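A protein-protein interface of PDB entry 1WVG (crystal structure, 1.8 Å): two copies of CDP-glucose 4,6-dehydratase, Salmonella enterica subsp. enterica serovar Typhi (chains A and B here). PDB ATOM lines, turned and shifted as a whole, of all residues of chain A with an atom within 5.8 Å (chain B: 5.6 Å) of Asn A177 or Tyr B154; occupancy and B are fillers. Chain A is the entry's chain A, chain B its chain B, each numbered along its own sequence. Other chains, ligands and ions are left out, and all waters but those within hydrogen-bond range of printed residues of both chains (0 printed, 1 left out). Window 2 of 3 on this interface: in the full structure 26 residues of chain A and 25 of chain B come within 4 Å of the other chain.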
ATOM      1  N   SER A 169      15.985   7.250 -12.609  1.00  0.00           N
ATOM      2  CA  SER A 169      14.964   8.164 -12.141  1.00  0.00           C
ATOM      3  C   SER A 169      14.028   7.546 -11.095  1.00  0.00           C
ATOM      4  O   SER A 169      13.470   8.231 -10.241  1.00  0.00           O
ATOM      5  CB  SER A 169      14.325   8.904 -13.309  1.00  0.00           C
ATOM      6  OG  SER A 169      13.446   8.091 -14.023  1.00  0.00           O
ATOM      7  N   ALA A 170      13.838   6.215 -11.137  1.00  0.00           N
ATOM      8  CA  ALA A 170      12.982   5.519 -10.178  1.00  0.00           C
ATOM      9  C   ALA A 170      13.702   5.431  -8.830  1.00  0.00           C
ATOM     10  O   ALA A 170      13.110   5.539  -7.750  1.00  0.00           O
ATOM     11  CB  ALA A 170      12.458   4.176 -10.691  1.00  0.00           C
ATOM     12  N   PHE A 171      15.027   5.258  -8.867  1.00  0.00           N
ATOM     13  CA  PHE A 171      15.748   5.222  -7.612  1.00  0.00           C
ATOM     14  C   PHE A 171      15.680   6.610  -7.005  1.00  0.00           C
ATOM     15  O   PHE A 171      15.419   6.794  -5.813  1.00  0.00           O
ATOM     16  CB  PHE A 171      17.214   4.800  -7.805  1.00  0.00           C
ATOM     17  CG  PHE A 171      17.383   3.323  -7.554  1.00  0.00           C
ATOM     18  CD1 PHE A 171      16.921   2.393  -8.486  1.00  0.00           C
ATOM     19  CD2 PHE A 171      17.977   2.848  -6.381  1.00  0.00           C
ATOM     20  CE1 PHE A 171      17.069   1.016  -8.278  1.00  0.00           C
ATOM     21  CE2 PHE A 171      18.118   1.475  -6.149  1.00  0.00           C
ATOM     22  CZ  PHE A 171      17.671   0.559  -7.104  1.00  0.00           C
ATOM     23  N   ARG A 172      15.915   7.587  -7.871  1.00  0.00           N
ATOM     24  CA  ARG A 172      15.865   8.938  -7.415  1.00  0.00           C
ATOM     25  C   ARG A 172      14.543   9.226  -6.756  1.00  0.00           C
ATOM     26  O   ARG A 172      14.515   9.728  -5.644  1.00  0.00           O
ATOM     27  CB  ARG A 172      16.063   9.949  -8.512  1.00  0.00           C
ATOM     28  CG  ARG A 172      16.149  11.364  -7.967  1.00  0.00           C
ATOM     29  CD  ARG A 172      16.374  12.397  -9.077  1.00  0.00           C
ATOM     30  NE  ARG A 172      17.535  12.219  -9.993  1.00  0.00           N
ATOM     31  CZ  ARG A 172      17.426  11.902 -11.308  1.00  0.00           C
ATOM     32  NH1 ARG A 172      16.238  11.687 -11.882  1.00  0.00           N
ATOM     33  NH2 ARG A 172      18.518  11.782 -12.087  1.00  0.00           N
ATOM     34  N   ASN A 173      13.452   8.904  -7.457  1.00  0.00           N
ATOM     35  CA  ASN A 173      12.091   9.136  -6.977  1.00  0.00           C
ATOM     36  C   ASN A 173      11.766   8.444  -5.673  1.00  0.00           C
ATOM     37  O   ASN A 173      11.302   9.067  -4.704  1.00  0.00           O
ATOM     38  CB  ASN A 173      10.998   8.801  -8.020  1.00  0.00           C
ATOM     39  CG  ASN A 173      10.740   9.941  -8.985  1.00  0.00           C
ATOM     40  OD1 ASN A 173      10.878  11.126  -8.614  1.00  0.00           O
ATOM     41  ND2 ASN A 173      10.364   9.591 -10.219  1.00  0.00           N
ATOM     42  N   SER A 174      12.022   7.165  -5.648  1.00  0.00           N
ATOM     43  CA  SER A 174      11.720   6.336  -4.500  1.00  0.00           C
ATOM     44  C   SER A 174      12.666   6.368  -3.323  1.00  0.00           C
ATOM     45  O   SER A 174      12.222   6.140  -2.188  1.00  0.00           O
ATOM     46  CB  SER A 174      11.747   4.884  -4.926  1.00  0.00           C
ATOM     47  OG  SER A 174      11.071   4.696  -6.140  1.00  0.00           O
ATOM     48  N   PHE A 175      13.957   6.552  -3.614  1.00  0.00           N
ATOM     49  CA  PHE A 175      14.935   6.499  -2.555  1.00  0.00           C
ATOM     50  C   PHE A 175      15.816   7.712  -2.302  1.00  0.00           C
ATOM     51  O   PHE A 175      16.297   7.889  -1.190  1.00  0.00           O
ATOM     52  CB  PHE A 175      15.778   5.250  -2.775  1.00  0.00           C
ATOM     53  CG  PHE A 175      14.983   3.996  -3.057  1.00  0.00           C
ATOM     54  CD1 PHE A 175      15.175   3.287  -4.244  1.00  0.00           C
ATOM     55  CD2 PHE A 175      14.072   3.477  -2.132  1.00  0.00           C
ATOM     56  CE1 PHE A 175      14.482   2.104  -4.519  1.00  0.00           C
ATOM     57  CE2 PHE A 175      13.359   2.307  -2.402  1.00  0.00           C
ATOM     58  CZ  PHE A 175      13.555   1.615  -3.599  1.00  0.00           C
ATOM     59  N   PHE A 176      16.070   8.518  -3.316  1.00  0.00           N
ATOM     60  CA  PHE A 176      16.907   9.708  -3.154  1.00  0.00           C
ATOM     61  C   PHE A 176      16.066  10.920  -3.523  1.00  0.00           C
ATOM     62  O   PHE A 176      16.493  11.798  -4.281  1.00  0.00           O
ATOM     63  CB  PHE A 176      18.156   9.646  -4.095  1.00  0.00           C
ATOM     64  CG  PHE A 176      18.882   8.318  -3.997  1.00  0.00           C
ATOM     65  CD1 PHE A 176      19.056   7.511  -5.126  1.00  0.00           C
ATOM     66  CD2 PHE A 176      19.392   7.851  -2.783  1.00  0.00           C
ATOM     67  CE1 PHE A 176      19.693   6.269  -5.049  1.00  0.00           C
ATOM     68  CE2 PHE A 176      20.043   6.616  -2.690  1.00  0.00           C
ATOM     69  CZ  PHE A 176      20.202   5.820  -3.829  1.00  0.00           C
ATOM     70  N   ASN A 177      14.827  10.949  -3.024  1.00  0.00           N
ATOM     71  CA  ASN A 177      13.942  12.018  -3.418  1.00  0.00           C
ATOM     72  C   ASN A 177      14.378  13.417  -3.007  1.00  0.00           C
ATOM     73  O   ASN A 177      14.602  13.701  -1.845  1.00  0.00           O
ATOM     74  CB  ASN A 177      12.505  11.707  -3.016  1.00  0.00           C
ATOM     75  CG  ASN A 177      11.533  12.555  -3.781  1.00  0.00           C
ATOM     76  OD1 ASN A 177      11.527  13.791  -3.719  1.00  0.00           O
ATOM     77  ND2 ASN A 177      10.728  11.876  -4.562  1.00  0.00           N
ATOM     78  N   PRO A 178      14.485  14.340  -3.954  1.00  0.00           N
ATOM     79  CA  PRO A 178      14.886  15.688  -3.566  1.00  0.00           C
ATOM     80  C   PRO A 178      14.124  16.218  -2.351  1.00  0.00           C
ATOM     81  O   PRO A 178      14.683  16.960  -1.550  1.00  0.00           O
ATOM     82  CB  PRO A 178      14.737  16.569  -4.813  1.00  0.00           C
ATOM     83  CG  PRO A 178      14.787  15.599  -5.998  1.00  0.00           C
ATOM     84  CD  PRO A 178      14.453  14.201  -5.446  1.00  0.00           C
ATOM     85  N   ALA A 179      12.852  15.811  -2.207  1.00  0.00           N
ATOM     86  CA  ALA A 179      11.976  16.213  -1.092  1.00  0.00           C
ATOM     87  C   ALA A 179      12.569  15.836   0.245  1.00  0.00           C
ATOM     88  O   ALA A 179      12.666  16.639   1.169  1.00  0.00           O
ATOM     89  CB  ALA A 179      10.597  15.566  -1.175  1.00  0.00           C
ATOM     90  N   ASN A 180      12.945  14.578   0.333  1.00  0.00           N
ATOM     91  CA  ASN A 180      13.533  14.057   1.539  1.00  0.00           C
ATOM     92  C   ASN A 180      15.049  14.117   1.481  1.00  0.00           C
ATOM     93  O   ASN A 180      15.728  13.309   2.116  1.00  0.00           O
ATOM     94  CB  ASN A 180      13.065  12.616   1.802  1.00  0.00           C
ATOM     95  CG  ASN A 180      12.723  11.911   0.511  1.00  0.00           C
ATOM     96  OD1 ASN A 180      11.543  11.659   0.241  1.00  0.00           O
ATOM     97  ND2 ASN A 180      13.734  11.653  -0.319  1.00  0.00           N
ATOM     98  N   TYR A 181      15.582  15.078   0.717  1.00  0.00           N
ATOM     99  CA  TYR A 181      17.030  15.209   0.582  1.00  0.00           C
ATOM    100  C   TYR A 181      17.803  15.145   1.898  1.00  0.00           C
ATOM    101  O   TYR A 181      18.817  14.440   2.040  1.00  0.00           O
ATOM    102  CB  TYR A 181      17.439  16.445  -0.238  1.00  0.00           C
ATOM    103  CG  TYR A 181      18.937  16.635  -0.405  1.00  0.00           C
ATOM    104  CD1 TYR A 181      19.829  15.585  -0.640  1.00  0.00           C
ATOM    105  CD2 TYR A 181      19.459  17.925  -0.360  1.00  0.00           C
ATOM    106  CE1 TYR A 181      21.198  15.815  -0.792  1.00  0.00           C
ATOM    107  CE2 TYR A 181      20.821  18.179  -0.517  1.00  0.00           C
ATOM    108  CZ  TYR A 181      21.700  17.117  -0.725  1.00  0.00           C
ATOM    109  OH  TYR A 181      23.043  17.394  -0.861  1.00  0.00           O
ATOM    110  N   HIS A 184      18.216  11.775   3.185  1.00  0.00           N
ATOM    111  CA  HIS A 184      19.159  10.843   2.567  1.00  0.00           C
ATOM    112  C   HIS A 184      20.521  11.444   2.217  1.00  0.00           C
ATOM    113  O   HIS A 184      21.546  10.771   2.231  1.00  0.00           O
ATOM    114  CB  HIS A 184      18.512  10.029   1.418  1.00  0.00           C
ATOM    115  CG  HIS A 184      17.997  10.950   0.373  1.00  0.00           C
ATOM    116  ND1 HIS A 184      16.644  11.129   0.205  1.00  0.00           N
ATOM    117  CD2 HIS A 184      18.672  11.761  -0.501  1.00  0.00           C
ATOM    118  CE1 HIS A 184      16.513  12.008  -0.768  1.00  0.00           C
ATOM    119  NE2 HIS A 184      17.702  12.412  -1.216  1.00  0.00           N
ATOM    120  N   TYR B  97       9.537  -1.717  -3.364  1.00  0.00           N
ATOM    121  CA  TYR B  97      10.351  -0.776  -2.593  1.00  0.00           C
ATOM    122  C   TYR B  97      11.387  -1.450  -1.714  1.00  0.00           C
ATOM    123  O   TYR B  97      12.474  -0.921  -1.498  1.00  0.00           O
ATOM    124  CB  TYR B  97       9.489   0.107  -1.677  1.00  0.00           C
ATOM    125  CG  TYR B  97       8.934   1.249  -2.446  1.00  0.00           C
ATOM    126  CD1 TYR B  97       7.685   1.146  -3.055  1.00  0.00           C
ATOM    127  CD2 TYR B  97       9.678   2.416  -2.613  1.00  0.00           C
ATOM    128  CE1 TYR B  97       7.156   2.208  -3.792  1.00  0.00           C
ATOM    129  CE2 TYR B  97       9.161   3.483  -3.350  1.00  0.00           C
ATOM    130  CZ  TYR B  97       7.896   3.385  -3.937  1.00  0.00           C
ATOM    131  OH  TYR B  97       7.366   4.447  -4.650  1.00  0.00           O
ATOM    132  N   GLY B 152       7.981   4.860 -18.420  1.00  0.00           N
ATOM    133  CA  GLY B 152       8.635   5.322 -17.206  1.00  0.00           C
ATOM    134  C   GLY B 152       8.159   4.523 -16.021  1.00  0.00           C
ATOM    135  O   GLY B 152       8.097   3.318 -16.026  1.00  0.00           O
ATOM    136  N   GLY B 153       7.750   5.214 -15.023  1.00  0.00           N
ATOM    137  CA  GLY B 153       7.284   4.535 -13.842  1.00  0.00           C
ATOM    138  C   GLY B 153       8.016   5.183 -12.683  1.00  0.00           C
ATOM    139  O   GLY B 153       9.234   5.405 -12.718  1.00  0.00           O
ATOM    140  N   TYR B 154       7.276   5.506 -11.645  1.00  0.00           N
ATOM    141  CA  TYR B 154       7.831   6.161 -10.472  1.00  0.00           C
ATOM    142  C   TYR B 154       8.520   5.253  -9.418  1.00  0.00           C
ATOM    143  O   TYR B 154       9.626   5.524  -8.935  1.00  0.00           O
ATOM    144  CB  TYR B 154       6.661   6.907  -9.876  1.00  0.00           C
ATOM    145  CG  TYR B 154       7.109   7.689  -8.705  1.00  0.00           C
ATOM    146  CD1 TYR B 154       7.459   9.032  -8.855  1.00  0.00           C
ATOM    147  CD2 TYR B 154       7.185   7.077  -7.453  1.00  0.00           C
ATOM    148  CE1 TYR B 154       7.869   9.772  -7.749  1.00  0.00           C
ATOM    149  CE2 TYR B 154       7.613   7.806  -6.345  1.00  0.00           C
ATOM    150  CZ  TYR B 154       7.953   9.151  -6.500  1.00  0.00           C
ATOM    151  OH  TYR B 154       8.352   9.885  -5.407  1.00  0.00           O
ATOM    152  N   ASP B 155       7.839   4.176  -9.033  1.00  0.00           N
ATOM    153  CA  ASP B 155       8.315   3.173  -8.084  1.00  0.00           C
ATOM    154  C   ASP B 155       9.012   2.017  -8.824  1.00  0.00           C
ATOM    155  O   ASP B 155       8.873   1.844 -10.047  1.00  0.00           O
ATOM    156  CB  ASP B 155       7.116   2.600  -7.307  1.00  0.00           C
ATOM    157  CG  ASP B 155       6.062   2.051  -8.237  1.00  0.00           C
ATOM    158  OD1 ASP B 155       5.273   2.778  -8.820  1.00  0.00           O
ATOM    159  OD2 ASP B 155       6.066   0.731  -8.333  1.00  0.00           O
ATOM    160  N   PRO B 156       9.764   1.176  -8.121  1.00  0.00           N
ATOM    161  CA  PRO B 156      10.437   0.138  -8.850  1.00  0.00           C
ATOM    162  C   PRO B 156       9.575  -0.798  -9.663  1.00  0.00           C
ATOM    163  O   PRO B 156       9.972  -1.245 -10.748  1.00  0.00           O
ATOM    164  CB  PRO B 156      11.332  -0.593  -7.864  1.00  0.00           C
ATOM    165  CG  PRO B 156      11.592   0.432  -6.773  1.00  0.00           C
ATOM    166  CD  PRO B 156      10.394   1.363  -6.794  1.00  0.00           C
ATOM    167  N   SER B 158       6.567  -0.226 -11.179  1.00  0.00           N
ATOM    168  CA  SER B 158       6.082   0.506 -12.340  1.00  0.00           C
ATOM    169  C   SER B 158       7.191   0.731 -13.300  1.00  0.00           C
ATOM    170  O   SER B 158       7.029   0.499 -14.497  1.00  0.00           O
ATOM    171  CB  SER B 158       5.592   1.852 -11.896  1.00  0.00           C
ATOM    172  OG  SER B 158       4.418   1.648 -11.128  1.00  0.00           O
ATOM    173  N   ASN B 159       8.325   1.179 -12.734  1.00  0.00           N
ATOM    174  CA  ASN B 159       9.514   1.422 -13.541  1.00  0.00           C
ATOM    175  C   ASN B 159      10.001   0.142 -14.228  1.00  0.00           C
ATOM    176  O   ASN B 159      10.424   0.161 -15.406  1.00  0.00           O
ATOM    177  CB  ASN B 159      10.609   2.137 -12.732  1.00  0.00           C
ATOM    178  CG  ASN B 159      11.734   2.751 -13.552  1.00  0.00           C
ATOM    179  OD1 ASN B 159      12.800   2.180 -13.713  1.00  0.00           O
ATOM    180  ND2 ASN B 159      11.538   3.967 -14.021  1.00  0.00           N
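O of Asn A173 lies within hydrogen-bond range of OH of Tyr B154 (3.1 Å). The side-chain hydroxyl (OG) of Ser A174 is in hydrogen-bond range of the backbone carbonyl oxygen (O) of Tyr B154 (3.3 Å). The side-chain amide nitrogen of Asn A177 lies within hydrogen-bond range of the side-chain hydroxyl of Tyr B154 (3.2 Å).
O of Ala A170 is in hydrogen-bond range of OG of Ser A174 (2.7 Å). N of Asn A177 lies within hydrogen-bond range of O of Arg A172, at 2.9 Å. ND2 of Asn A177 is in hydrogen-bond range of O of Asn A173 (2.9 Å). The backbone NH (N) of Ala A179 lies within hydrogen-bond range of the side-chain amide oxygen (OD1) of Asn A177, at 2.8 Å. O of Asn A177 is in hydrogen-bond range of ND2 of Asn A180 (2.7 Å). The backbone carbonyl oxygen (O) of Asn A177 lies close to a ring nitrogen (NE2) of His A184.
CA of Ala A170 touches O of Tyr B154, at 3.6 Å. CB of Ala A170 touches CG of Asn B159, 3.3 Å away. CE2 of Tyr B97 touches CB of Ser A174 (3.3 Å). OG of Ser A174 touches CA of Asp B155, 3.7 Å away. Pro B156 touches Ser A174 (CD to OG, 3.5 Å). Tyr B97 touches Phe A175. Pro B156 touches Phe A175.
Of the printed residues of chain A, Tyr B97 touches Ser A174 and Phe A175. Printed residues of chain B within 4 Å of Ala A170: Tyr B154 and Asn B159. Printed residues of chain B within 4 Å of Asn A173: Tyr B154 (3.1 Å). The nearest printed residue of chain A that does not touch Tyr B154 is Ser A169 (4.9 Å).
Printed residues of chain A that touch a printed residue of chain B: Ala A170, Asn A173, Ser A174, Phe A175 and Asn A177. Hydrophobic or aromatic side chains of chain A within 4 Å of the printed part of chain B: Ala A170 and Phe A175. Along chain A the printed residues that touch a printed residue of chain B span positions 170 to 177.
No position is printed for both chains.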
